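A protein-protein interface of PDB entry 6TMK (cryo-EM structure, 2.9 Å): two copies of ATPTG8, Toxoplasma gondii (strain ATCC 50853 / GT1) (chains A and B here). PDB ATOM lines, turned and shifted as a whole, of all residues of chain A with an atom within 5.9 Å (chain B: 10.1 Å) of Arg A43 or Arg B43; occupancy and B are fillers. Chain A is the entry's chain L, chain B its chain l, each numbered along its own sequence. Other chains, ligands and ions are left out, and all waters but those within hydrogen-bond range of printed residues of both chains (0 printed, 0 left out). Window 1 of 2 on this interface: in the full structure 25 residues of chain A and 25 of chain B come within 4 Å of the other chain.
Among the printed residues, 5 pairs touch across the chains.
Arg A43 touches two residues of chain B.
Arg B43 touches just these residues of chain A: Arg A43 (3.7 Å) and Glu A44 (3.8 Å).
Of chain B, only Glu B44 (3.6 Å) comes within 4 Å of Asn A40.
Of the printed residues of chain A, Glu B44 touches Asn A40 and Arg A43.
Of the printed residues of chain A, Asn B40 touches Glu A44.
Leu B45 touches none of the printed residues of chain A.
The nearest residue of chain B that does not touch Arg A43 is Asn B40 (4.6 Å).
ND2 of Asn B40 is in hydrogen-bond range of OE1 of Glu B44 (3.3 Å).
NH2 of Arg B190 lies within salt-bridge range of OE2 of Glu B44 (2.4 Å).
The side-chain carboxylate of Glu A44 lies within hydrogen-bond range of the side-chain amide nitrogen of Asn A40, 3.2 Å away.
Asn A40 touches Glu B44, and with the chains exchanged Glu A44 touches Asn B40.
Arg A43 touches its own counterpart, Arg B43.
Arg A43 touches Glu B44, and with the chains exchanged Glu A44 touches Arg B43.
11 positions are printed for both chains.
Of the 5 pairs that touch across the chains among the printed residues, 5 have their exchanged pair printed and touching as well.
Among the printed residues, merely in contact across the chains: Asn A40 with Glu B44, Arg A43 with Arg B43, Arg A43 with Glu B44, Glu A44 with Asn B40 and Glu A44 with Arg B43.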
ATOM      1  N   LEU A  38     -11.827 -21.150  -2.203  1.00  0.00           N
ATOM      2  CA  LEU A  38     -10.409 -21.077  -1.885  1.00  0.00           C
ATOM      3  C   LEU A  38     -10.017 -19.687  -1.421  1.00  0.00           C
ATOM      4  O   LEU A  38      -9.252 -19.539  -0.461  1.00  0.00           O
ATOM      5  CB  LEU A  38      -9.578 -21.468  -3.100  1.00  0.00           C
ATOM      6  CG  LEU A  38      -9.491 -22.943  -3.454  1.00  0.00           C
ATOM      7  CD1 LEU A  38      -8.636 -23.088  -4.682  1.00  0.00           C
ATOM      8  CD2 LEU A  38      -8.918 -23.737  -2.313  1.00  0.00           C
ATOM      9  N   GLN A  39     -10.497 -18.653  -2.108  1.00  0.00           N
ATOM     10  CA  GLN A  39     -10.101 -17.305  -1.727  1.00  0.00           C
ATOM     11  C   GLN A  39     -10.680 -16.929  -0.366  1.00  0.00           C
ATOM     12  O   GLN A  39     -10.017 -16.253   0.430  1.00  0.00           O
ATOM     13  CB  GLN A  39     -10.529 -16.305  -2.799  1.00  0.00           C
ATOM     14  CG  GLN A  39     -11.978 -15.913  -2.767  1.00  0.00           C
ATOM     15  CD  GLN A  39     -12.292 -14.798  -3.733  1.00  0.00           C
ATOM     16  OE1 GLN A  39     -11.456 -14.413  -4.549  1.00  0.00           O
ATOM     17  NE2 GLN A  39     -13.495 -14.253  -3.631  1.00  0.00           N
ATOM     18  N   ASN A  40     -11.895 -17.390  -0.060  1.00  0.00           N
ATOM     19  CA  ASN A  40     -12.441 -17.153   1.274  1.00  0.00           C
ATOM     20  C   ASN A  40     -11.592 -17.842   2.341  1.00  0.00           C
ATOM     21  O   ASN A  40     -11.294 -17.259   3.398  1.00  0.00           O
ATOM     22  CB  ASN A  40     -13.891 -17.632   1.339  1.00  0.00           C
ATOM     23  CG  ASN A  40     -14.443 -17.640   2.749  1.00  0.00           C
ATOM     24  OD1 ASN A  40     -14.638 -16.588   3.356  1.00  0.00           O
ATOM     25  ND2 ASN A  40     -14.705 -18.831   3.277  1.00  0.00           N
ATOM     26  N   ILE A  41     -11.191 -19.085   2.075  1.00  0.00           N
ATOM     27  CA  ILE A  41     -10.340 -19.819   3.007  1.00  0.00           C
ATOM     28  C   ILE A  41      -9.029 -19.079   3.230  1.00  0.00           C
ATOM     29  O   ILE A  41      -8.548 -18.960   4.366  1.00  0.00           O
ATOM     30  CB  ILE A  41     -10.096 -21.243   2.479  1.00  0.00           C
ATOM     31  CG1 ILE A  41     -11.400 -22.029   2.418  1.00  0.00           C
ATOM     32  CG2 ILE A  41      -9.106 -21.959   3.350  1.00  0.00           C
ATOM     33  CD1 ILE A  41     -11.881 -22.511   3.742  1.00  0.00           C
ATOM     34  N   GLU A  42      -8.418 -18.593   2.152  1.00  0.00           N
ATOM     35  CA  GLU A  42      -7.152 -17.882   2.270  1.00  0.00           C
ATOM     36  C   GLU A  42      -7.318 -16.597   3.066  1.00  0.00           C
ATOM     37  O   GLU A  42      -6.429 -16.212   3.829  1.00  0.00           O
ATOM     38  CB  GLU A  42      -6.581 -17.582   0.890  1.00  0.00           C
ATOM     39  CG  GLU A  42      -6.091 -18.804   0.156  1.00  0.00           C
ATOM     40  CD  GLU A  42      -5.713 -18.511  -1.278  1.00  0.00           C
ATOM     41  OE1 GLU A  42      -5.690 -17.321  -1.656  1.00  0.00           O
ATOM     42  OE2 GLU A  42      -5.439 -19.470  -2.029  1.00  0.00           O
ATOM     43  N   ARG A  43      -8.450 -15.917   2.895  1.00  0.00           N
ATOM     44  CA  ARG A  43      -8.720 -14.722   3.684  1.00  0.00           C
ATOM     45  C   ARG A  43      -8.763 -15.049   5.171  1.00  0.00           C
ATOM     46  O   ARG A  43      -8.165 -14.347   5.998  1.00  0.00           O
ATOM     47  CB  ARG A  43     -10.030 -14.098   3.219  1.00  0.00           C
ATOM     48  CG  ARG A  43     -10.232 -12.675   3.652  1.00  0.00           C
ATOM     49  CD  ARG A  43     -11.550 -12.126   3.155  1.00  0.00           C
ATOM     50  NE  ARG A  43     -12.677 -12.945   3.600  1.00  0.00           N
ATOM     51  CZ  ARG A  43     -13.491 -13.636   2.800  1.00  0.00           C
ATOM     52  NH1 ARG A  43     -13.336 -13.627   1.478  1.00  0.00           N
ATOM     53  NH2 ARG A  43     -14.477 -14.345   3.333  1.00  0.00           N
ATOM     54  N   GLU A  44      -9.473 -16.117   5.531  1.00  0.00           N
ATOM     55  CA  GLU A  44      -9.548 -16.509   6.937  1.00  0.00           C
ATOM     56  C   GLU A  44      -8.166 -16.848   7.488  1.00  0.00           C
ATOM     57  O   GLU A  44      -7.789 -16.414   8.589  1.00  0.00           O
ATOM     58  CB  GLU A  44     -10.491 -17.696   7.096  1.00  0.00           C
ATOM     59  CG  GLU A  44     -11.946 -17.317   7.158  1.00  0.00           C
ATOM     60  CD  GLU A  44     -12.868 -18.506   6.994  1.00  0.00           C
ATOM     61  OE1 GLU A  44     -12.840 -19.139   5.918  1.00  0.00           O
ATOM     62  OE2 GLU A  44     -13.625 -18.808   7.941  1.00  0.00           O
ATOM     63  N   LEU A  45      -7.404 -17.645   6.739  1.00  0.00           N
ATOM     64  CA  LEU A  45      -6.059 -18.005   7.171  1.00  0.00           C
ATOM     65  C   LEU A  45      -5.187 -16.773   7.357  1.00  0.00           C
ATOM     66  O   LEU A  45      -4.403 -16.698   8.307  1.00  0.00           O
ATOM     67  CB  LEU A  45      -5.418 -18.944   6.159  1.00  0.00           C
ATOM     68  CG  LEU A  45      -5.768 -20.420   6.246  1.00  0.00           C
ATOM     69  CD1 LEU A  45      -5.401 -21.100   4.956  1.00  0.00           C
ATOM     70  CD2 LEU A  45      -5.051 -21.052   7.403  1.00  0.00           C
ATOM     71  N   LYS A  46      -5.290 -15.809   6.443  1.00  0.00           N
ATOM     72  CA  LYS A  46      -4.506 -14.591   6.560  1.00  0.00           C
ATOM     73  C   LYS A  46      -4.869 -13.822   7.815  1.00  0.00           C
ATOM     74  O   LYS A  46      -3.990 -13.303   8.508  1.00  0.00           O
ATOM     75  CB  LYS A  46      -4.710 -13.720   5.330  1.00  0.00           C
ATOM     76  CG  LYS A  46      -3.737 -12.591   5.238  1.00  0.00           C
ATOM     77  CD  LYS A  46      -4.147 -11.589   4.206  1.00  0.00           C
ATOM     78  CE  LYS A  46      -3.278 -10.372   4.271  1.00  0.00           C
ATOM     79  NZ  LYS A  46      -3.300  -9.607   3.023  1.00  0.00           N
ATOM     80  N   ASP A  47      -6.159 -13.730   8.122  1.00  0.00           N
ATOM     81  CA  ASP A  47      -6.563 -13.018   9.326  1.00  0.00           C
ATOM     82  C   ASP A  47      -5.951 -13.671  10.555  1.00  0.00           C
ATOM     83  O   ASP A  47      -5.335 -12.999  11.397  1.00  0.00           O
ATOM     84  CB  ASP A  47      -8.084 -12.963   9.430  1.00  0.00           C
ATOM     85  CG  ASP A  47      -8.575 -11.710  10.130  1.00  0.00           C
ATOM     86  OD1 ASP A  47      -7.830 -11.166  10.971  1.00  0.00           O
ATOM     87  OD2 ASP A  47      -9.702 -11.262   9.837  1.00  0.00           O
ATOM     88  N   TRP A  48      -6.086 -14.993  10.660  1.00  0.00           N
ATOM     89  CA  TRP A  48      -5.494 -15.703  11.787  1.00  0.00           C
ATOM     90  C   TRP A  48      -3.998 -15.447  11.877  1.00  0.00           C
ATOM     91  O   TRP A  48      -3.481 -15.069  12.936  1.00  0.00           O
ATOM     92  CB  TRP A  48      -5.763 -17.200  11.671  1.00  0.00           C
ATOM     93  CG  TRP A  48      -4.932 -18.006  12.604  1.00  0.00           C
ATOM     94  CD1 TRP A  48      -5.172 -18.230  13.917  1.00  0.00           C
ATOM     95  CD2 TRP A  48      -3.714 -18.694  12.297  1.00  0.00           C
ATOM     96  NE1 TRP A  48      -4.183 -19.012  14.454  1.00  0.00           N
ATOM     97  CE2 TRP A  48      -3.276 -19.309  13.476  1.00  0.00           C
ATOM     98  CE3 TRP A  48      -2.952 -18.845  11.140  1.00  0.00           C
ATOM     99  CZ2 TRP A  48      -2.118 -20.062  13.533  1.00  0.00           C
ATOM    100  CZ3 TRP A  48      -1.805 -19.590  11.203  1.00  0.00           C
ATOM    101  CH2 TRP A  48      -1.398 -20.188  12.387  1.00  0.00           C
ATOM    102  N   LYS B  35     -20.210 -17.009  17.993  1.00  0.00           N
ATOM    103  CA  LYS B  35     -20.033 -15.595  17.686  1.00  0.00           C
ATOM    104  C   LYS B  35     -19.027 -15.400  16.559  1.00  0.00           C
ATOM    105  O   LYS B  35     -19.225 -14.558  15.672  1.00  0.00           O
ATOM    106  CB  LYS B  35     -19.578 -14.855  18.939  1.00  0.00           C
ATOM    107  CG  LYS B  35     -20.584 -14.894  20.063  1.00  0.00           C
ATOM    108  CD  LYS B  35     -21.544 -13.734  20.009  1.00  0.00           C
ATOM    109  CE  LYS B  35     -22.559 -13.840  21.124  1.00  0.00           C
ATOM    110  NZ  LYS B  35     -21.941 -13.610  22.455  1.00  0.00           N
ATOM    111  N   LEU B  36     -17.937 -16.164  16.582  1.00  0.00           N
ATOM    112  CA  LEU B  36     -16.946 -16.054  15.517  1.00  0.00           C
ATOM    113  C   LEU B  36     -17.531 -16.479  14.173  1.00  0.00           C
ATOM    114  O   LEU B  36     -17.318 -15.816  13.146  1.00  0.00           O
ATOM    115  CB  LEU B  36     -15.719 -16.893  15.855  1.00  0.00           C
ATOM    116  CG  LEU B  36     -14.902 -16.421  17.053  1.00  0.00           C
ATOM    117  CD1 LEU B  36     -13.759 -17.369  17.271  1.00  0.00           C
ATOM    118  CD2 LEU B  36     -14.395 -15.007  16.860  1.00  0.00           C
ATOM    119  N   GLU B  37     -18.280 -17.581  14.168  1.00  0.00           N
ATOM    120  CA  GLU B  37     -18.969 -17.997  12.953  1.00  0.00           C
ATOM    121  C   GLU B  37     -19.890 -16.898  12.443  1.00  0.00           C
ATOM    122  O   GLU B  37     -19.922 -16.604  11.242  1.00  0.00           O
ATOM    123  CB  GLU B  37     -19.753 -19.279  13.217  1.00  0.00           C
ATOM    124  CG  GLU B  37     -20.246 -19.973  11.970  1.00  0.00           C
ATOM    125  CD  GLU B  37     -19.140 -20.675  11.211  1.00  0.00           C
ATOM    126  OE1 GLU B  37     -17.988 -20.673  11.696  1.00  0.00           O
ATOM    127  OE2 GLU B  37     -19.423 -21.230  10.129  1.00  0.00           O
ATOM    128  N   LEU B  38     -20.642 -16.276  13.348  1.00  0.00           N
ATOM    129  CA  LEU B  38     -21.575 -15.229  12.957  1.00  0.00           C
ATOM    130  C   LEU B  38     -20.851 -14.057  12.318  1.00  0.00           C
ATOM    131  O   LEU B  38     -21.311 -13.510  11.311  1.00  0.00           O
ATOM    132  CB  LEU B  38     -22.364 -14.749  14.167  1.00  0.00           C
ATOM    133  CG  LEU B  38     -23.480 -15.641  14.685  1.00  0.00           C
ATOM    134  CD1 LEU B  38     -24.104 -14.978  15.880  1.00  0.00           C
ATOM    135  CD2 LEU B  38     -24.510 -15.884  13.617  1.00  0.00           C
ATOM    136  N   GLN B  39     -19.738 -13.631  12.908  1.00  0.00           N
ATOM    137  CA  GLN B  39     -19.044 -12.475  12.359  1.00  0.00           C
ATOM    138  C   GLN B  39     -18.440 -12.795  10.996  1.00  0.00           C
ATOM    139  O   GLN B  39     -18.438 -11.943  10.098  1.00  0.00           O
ATOM    140  CB  GLN B  39     -17.972 -11.989  13.333  1.00  0.00           C
ATOM    141  CG  GLN B  39     -16.699 -12.785  13.329  1.00  0.00           C
ATOM    142  CD  GLN B  39     -15.625 -12.153  14.179  1.00  0.00           C
ATOM    143  OE1 GLN B  39     -15.874 -11.190  14.903  1.00  0.00           O
ATOM    144  NE2 GLN B  39     -14.412 -12.675  14.077  1.00  0.00           N
ATOM    145  N   ASN B  40     -17.958 -14.024  10.803  1.00  0.00           N
ATOM    146  CA  ASN B  40     -17.477 -14.411   9.479  1.00  0.00           C
ATOM    147  C   ASN B  40     -18.611 -14.376   8.456  1.00  0.00           C
ATOM    148  O   ASN B  40     -18.440 -13.882   7.328  1.00  0.00           O
ATOM    149  CB  ASN B  40     -16.840 -15.798   9.538  1.00  0.00           C
ATOM    150  CG  ASN B  40     -16.538 -16.364   8.167  1.00  0.00           C
ATOM    151  OD1 ASN B  40     -15.667 -15.864   7.457  1.00  0.00           O
ATOM    152  ND2 ASN B  40     -17.253 -17.417   7.789  1.00  0.00           N
ATOM    153  N   ILE B  41     -19.778 -14.893   8.838  1.00  0.00           N
ATOM    154  CA  ILE B  41     -20.937 -14.873   7.953  1.00  0.00           C
ATOM    155  C   ILE B  41     -21.304 -13.442   7.585  1.00  0.00           C
ATOM    156  O   ILE B  41     -21.601 -13.138   6.422  1.00  0.00           O
ATOM    157  CB  ILE B  41     -22.118 -15.597   8.623  1.00  0.00           C
ATOM    158  CG1 ILE B  41     -21.797 -17.073   8.833  1.00  0.00           C
ATOM    159  CG2 ILE B  41     -23.359 -15.456   7.790  1.00  0.00           C
ATOM    160  CD1 ILE B  41     -21.886 -17.895   7.596  1.00  0.00           C
ATOM    161  N   GLU B  42     -21.317 -12.548   8.573  1.00  0.00           N
ATOM    162  CA  GLU B  42     -21.669 -11.158   8.313  1.00  0.00           C
ATOM    163  C   GLU B  42     -20.656 -10.502   7.387  1.00  0.00           C
ATOM    164  O   GLU B  42     -21.019  -9.677   6.545  1.00  0.00           O
ATOM    165  CB  GLU B  42     -21.773 -10.384   9.620  1.00  0.00           C
ATOM    166  CG  GLU B  42     -22.963 -10.765  10.461  1.00  0.00           C
ATOM    167  CD  GLU B  42     -22.938 -10.127  11.831  1.00  0.00           C
ATOM    168  OE1 GLU B  42     -22.069  -9.263  12.070  1.00  0.00           O
ATOM    169  OE2 GLU B  42     -23.786 -10.491  12.674  1.00  0.00           O
ATOM    170  N   ARG B  43     -19.380 -10.851   7.534  1.00  0.00           N
ATOM    171  CA  ARG B  43     -18.361 -10.331   6.631  1.00  0.00           C
ATOM    172  C   ARG B  43     -18.646 -10.748   5.193  1.00  0.00           C
ATOM    173  O   ARG B  43     -18.581  -9.929   4.265  1.00  0.00           O
ATOM    174  CB  ARG B  43     -16.991 -10.817   7.084  1.00  0.00           C
ATOM    175  CG  ARG B  43     -15.835 -10.055   6.504  1.00  0.00           C
ATOM    176  CD  ARG B  43     -14.512 -10.595   6.998  1.00  0.00           C
ATOM    177  NE  ARG B  43     -14.367 -12.019   6.700  1.00  0.00           N
ATOM    178  CZ  ARG B  43     -14.277 -12.991   7.608  1.00  0.00           C
ATOM    179  NH1 ARG B  43     -14.310 -12.727   8.911  1.00  0.00           N
ATOM    180  NH2 ARG B  43     -14.149 -14.247   7.203  1.00  0.00           N
ATOM    181  N   GLU B  44     -18.960 -12.026   4.990  1.00  0.00           N
ATOM    182  CA  GLU B  44     -19.264 -12.502   3.642  1.00  0.00           C
ATOM    183  C   GLU B  44     -20.482 -11.784   3.067  1.00  0.00           C
ATOM    184  O   GLU B  44     -20.477 -11.339   1.906  1.00  0.00           O
ATOM    185  CB  GLU B  44     -19.495 -14.007   3.662  1.00  0.00           C
ATOM    186  CG  GLU B  44     -18.227 -14.820   3.625  1.00  0.00           C
ATOM    187  CD  GLU B  44     -18.456 -16.277   3.969  1.00  0.00           C
ATOM    188  OE1 GLU B  44     -18.885 -16.561   5.107  1.00  0.00           O
ATOM    189  OE2 GLU B  44     -18.204 -17.140   3.102  1.00  0.00           O
ATOM    190  N   LEU B  45     -21.546 -11.680   3.863  1.00  0.00           N
ATOM    191  CA  LEU B  45     -22.746 -10.987   3.409  1.00  0.00           C
ATOM    192  C   LEU B  45     -22.449  -9.542   3.046  1.00  0.00           C
ATOM    193  O   LEU B  45     -22.976  -9.023   2.057  1.00  0.00           O
ATOM    194  CB  LEU B  45     -23.819 -11.040   4.488  1.00  0.00           C
ATOM    195  CG  LEU B  45     -24.661 -12.302   4.583  1.00  0.00           C
ATOM    196  CD1 LEU B  45     -25.346 -12.349   5.920  1.00  0.00           C
ATOM    197  CD2 LEU B  45     -25.665 -12.336   3.470  1.00  0.00           C
ATOM    198  N   LYS B  46     -21.628  -8.867   3.849  1.00  0.00           N
ATOM    199  CA  LYS B  46     -21.281  -7.485   3.558  1.00  0.00           C
ATOM    200  C   LYS B  46     -20.537  -7.373   2.241  1.00  0.00           C
ATOM    201  O   LYS B  46     -20.792  -6.459   1.453  1.00  0.00           O
ATOM    202  CB  LYS B  46     -20.444  -6.909   4.689  1.00  0.00           C
ATOM    203  CG  LYS B  46     -20.281  -5.426   4.607  1.00  0.00           C
ATOM    204  CD  LYS B  46     -19.222  -4.933   5.539  1.00  0.00           C
ATOM    205  CE  LYS B  46     -18.930  -3.486   5.295  1.00  0.00           C
ATOM    206  NZ  LYS B  46     -18.296  -2.845   6.447  1.00  0.00           N
ATOM    207  N   ASP B  47     -19.606  -8.288   1.988  1.00  0.00           N
ATOM    208  CA  ASP B  47     -18.870  -8.239   0.732  1.00  0.00           C
ATOM    209  C   ASP B  47     -19.825  -8.370  -0.445  1.00  0.00           C
ATOM    210  O   ASP B  47     -19.794  -7.561  -1.385  1.00  0.00           O
ATOM    211  CB  ASP B  47     -17.801  -9.326   0.698  1.00  0.00           C
ATOM    212  CG  ASP B  47     -16.582  -8.918  -0.106  1.00  0.00           C
ATOM    213  OD1 ASP B  47     -16.726  -8.091  -1.032  1.00  0.00           O
ATOM    214  OD2 ASP B  47     -15.476  -9.420   0.183  1.00  0.00           O
ATOM    215  N   TRP B  48     -20.704  -9.370  -0.393  1.00  0.00           N
ATOM    216  CA  TRP B  48     -21.683  -9.542  -1.458  1.00  0.00           C
ATOM    217  C   TRP B  48     -22.521  -8.286  -1.648  1.00  0.00           C
ATOM    218  O   TRP B  48     -22.649  -7.772  -2.766  1.00  0.00           O
ATOM    219  CB  TRP B  48     -22.586 -10.735  -1.160  1.00  0.00           C
ATOM    220  CG  TRP B  48     -23.790 -10.774  -2.035  1.00  0.00           C
ATOM    221  CD1 TRP B  48     -23.857 -11.245  -3.302  1.00  0.00           C
ATOM    222  CD2 TRP B  48     -25.105 -10.313  -1.709  1.00  0.00           C
ATOM    223  NE1 TRP B  48     -25.129 -11.110  -3.792  1.00  0.00           N
ATOM    224  CE2 TRP B  48     -25.914 -10.538  -2.831  1.00  0.00           C
ATOM    225  CE3 TRP B  48     -25.676  -9.729  -0.580  1.00  0.00           C
ATOM    226  CZ2 TRP B  48     -27.256 -10.204  -2.855  1.00  0.00           C
ATOM    227  CZ3 TRP B  48     -27.006  -9.399  -0.611  1.00  0.00           C
ATOM    228  CH2 TRP B  48     -27.780  -9.636  -1.737  1.00  0.00           C
ATOM    229  N   TRP B  49     -23.112  -7.789  -0.567  1.00  0.00           N
ATOM    230  CA  TRP B  49     -24.040  -6.676  -0.676  1.00  0.00           C
ATOM    231  C   TRP B  49     -23.352  -5.434  -1.216  1.00  0.00           C
ATOM    232  O   TRP B  49     -23.905  -4.733  -2.069  1.00  0.00           O
ATOM    233  CB  TRP B  49     -24.656  -6.402   0.690  1.00  0.00           C
ATOM    234  CG  TRP B  49     -25.803  -5.475   0.671  1.00  0.00           C
ATOM    235  CD1 TRP B  49     -27.104  -5.800   0.496  1.00  0.00           C
ATOM    236  CD2 TRP B  49     -25.762  -4.062   0.850  1.00  0.00           C
ATOM    237  NE1 TRP B  49     -27.882  -4.680   0.547  1.00  0.00           N
ATOM    238  CE2 TRP B  49     -27.078  -3.596   0.765  1.00  0.00           C
ATOM    239  CE3 TRP B  49     -24.739  -3.144   1.073  1.00  0.00           C
ATOM    240  CZ2 TRP B  49     -27.397  -2.258   0.890  1.00  0.00           C
ATOM    241  CZ3 TRP B  49     -25.059  -1.824   1.194  1.00  0.00           C
ATOM    242  CH2 TRP B  49     -26.374  -1.390   1.105  1.00  0.00           C
ATOM    243  N   MET B  50     -22.143  -5.143  -0.742  1.00  0.00           N
ATOM    244  CA  MET B  50     -21.484  -3.914  -1.153  1.00  0.00           C
ATOM    245  C   MET B  50     -21.025  -3.999  -2.599  1.00  0.00           C
ATOM    246  O   MET B  50     -21.140  -3.020  -3.346  1.00  0.00           O
ATOM    247  CB  MET B  50     -20.310  -3.614  -0.230  1.00  0.00           C
ATOM    248  CG  MET B  50     -20.696  -3.382   1.205  1.00  0.00           C
ATOM    249  SD  MET B  50     -21.326  -1.734   1.500  1.00  0.00           S
ATOM    250  CE  MET B  50     -19.778  -0.888   1.702  1.00  0.00           C
ATOM    251  N   SER B  51     -20.522  -5.159  -3.025  1.00  0.00           N
ATOM    252  CA  SER B  51     -20.159  -5.313  -4.426  1.00  0.00           C
ATOM    253  C   SER B  51     -21.379  -5.141  -5.318  1.00  0.00           C
ATOM    254  O   SER B  51     -21.334  -4.426  -6.328  1.00  0.00           O
ATOM    255  CB  SER B  51     -19.506  -6.675  -4.643  1.00  0.00           C
ATOM    256  OG  SER B  51     -18.526  -6.933  -3.659  1.00  0.00           O
ATOM    257  N   ARG B 190     -26.000 -18.121  -2.749  1.00  0.00           N
ATOM    258  CA  ARG B 190     -25.073 -18.328  -1.645  1.00  0.00           C
ATOM    259  C   ARG B 190     -25.349 -17.353  -0.509  1.00  0.00           C
ATOM    260  O   ARG B 190     -25.333 -17.733   0.670  1.00  0.00           O
ATOM    261  CB  ARG B 190     -23.637 -18.188  -2.137  1.00  0.00           C
ATOM    262  CG  ARG B 190     -22.607 -18.597  -1.125  1.00  0.00           C
ATOM    263  CD  ARG B 190     -21.222 -18.624  -1.724  1.00  0.00           C
ATOM    264  NE  ARG B 190     -20.186 -18.637  -0.696  1.00  0.00           N
ATOM    265  CZ  ARG B 190     -19.712 -17.551  -0.095  1.00  0.00           C
ATOM    266  NH1 ARG B 190     -20.175 -16.352  -0.410  1.00  0.00           N
ATOM    267  NH2 ARG B 190     -18.771 -17.665   0.830  1.00  0.00           N
ATOM    268  N   ALA B 191     -25.597 -16.089  -0.844  1.00  0.00           N
ATOM    269  CA  ALA B 191     -25.878 -15.096   0.184  1.00  0.00           C
ATOM    270  C   ALA B 191     -27.149 -15.436   0.950  1.00  0.00           C
ATOM    271  O   ALA B 191     -27.204 -15.289   2.176  1.00  0.00           O
ATOM    272  CB  ALA B 191     -25.991 -13.719  -0.453  1.00  0.00           C
ATOM    273  N   LEU B 194     -26.384 -18.190   3.382  1.00  0.00           N
ATOM    274  CA  LEU B 194     -25.661 -17.640   4.524  1.00  0.00           C
ATOM    275  C   LEU B 194     -26.600 -16.908   5.470  1.00  0.00           C
ATOM    276  O   LEU B 194     -26.441 -16.973   6.695  1.00  0.00           O
ATOM    277  CB  LEU B 194     -24.566 -16.694   4.045  1.00  0.00           C
ATOM    278  CG  LEU B 194     -23.372 -17.282   3.303  1.00  0.00           C
ATOM    279  CD1 LEU B 194     -22.372 -16.193   3.045  1.00  0.00           C
ATOM    280  CD2 LEU B 194     -22.731 -18.395   4.089  1.00  0.00           C
ATOM    281  N   ARG B 198     -27.201 -17.763   9.392  1.00  0.00           N
ATOM    282  CA  ARG B 198     -27.126 -16.757  10.442  1.00  0.00           C
ATOM    283  C   ARG B 198     -28.392 -16.744  11.280  1.00  0.00           C
ATOM    284  O   ARG B 198     -28.336 -16.548  12.498  1.00  0.00           O
ATOM    285  CB  ARG B 198     -26.886 -15.386   9.828  1.00  0.00           C
ATOM    286  CG  ARG B 198     -26.765 -14.281  10.831  1.00  0.00           C
ATOM    287  CD  ARG B 198     -26.279 -13.023  10.184  1.00  0.00           C
ATOM    288  NE  ARG B 198     -26.327 -11.879  11.083  1.00  0.00           N
ATOM    289  CZ  ARG B 198     -27.404 -11.134  11.286  1.00  0.00           C
ATOM    290  NH1 ARG B 198     -28.537 -11.403  10.661  1.00  0.00           N
ATOM    291  NH2 ARG B 198     -27.349 -10.115  12.119  1.00  0.00           N
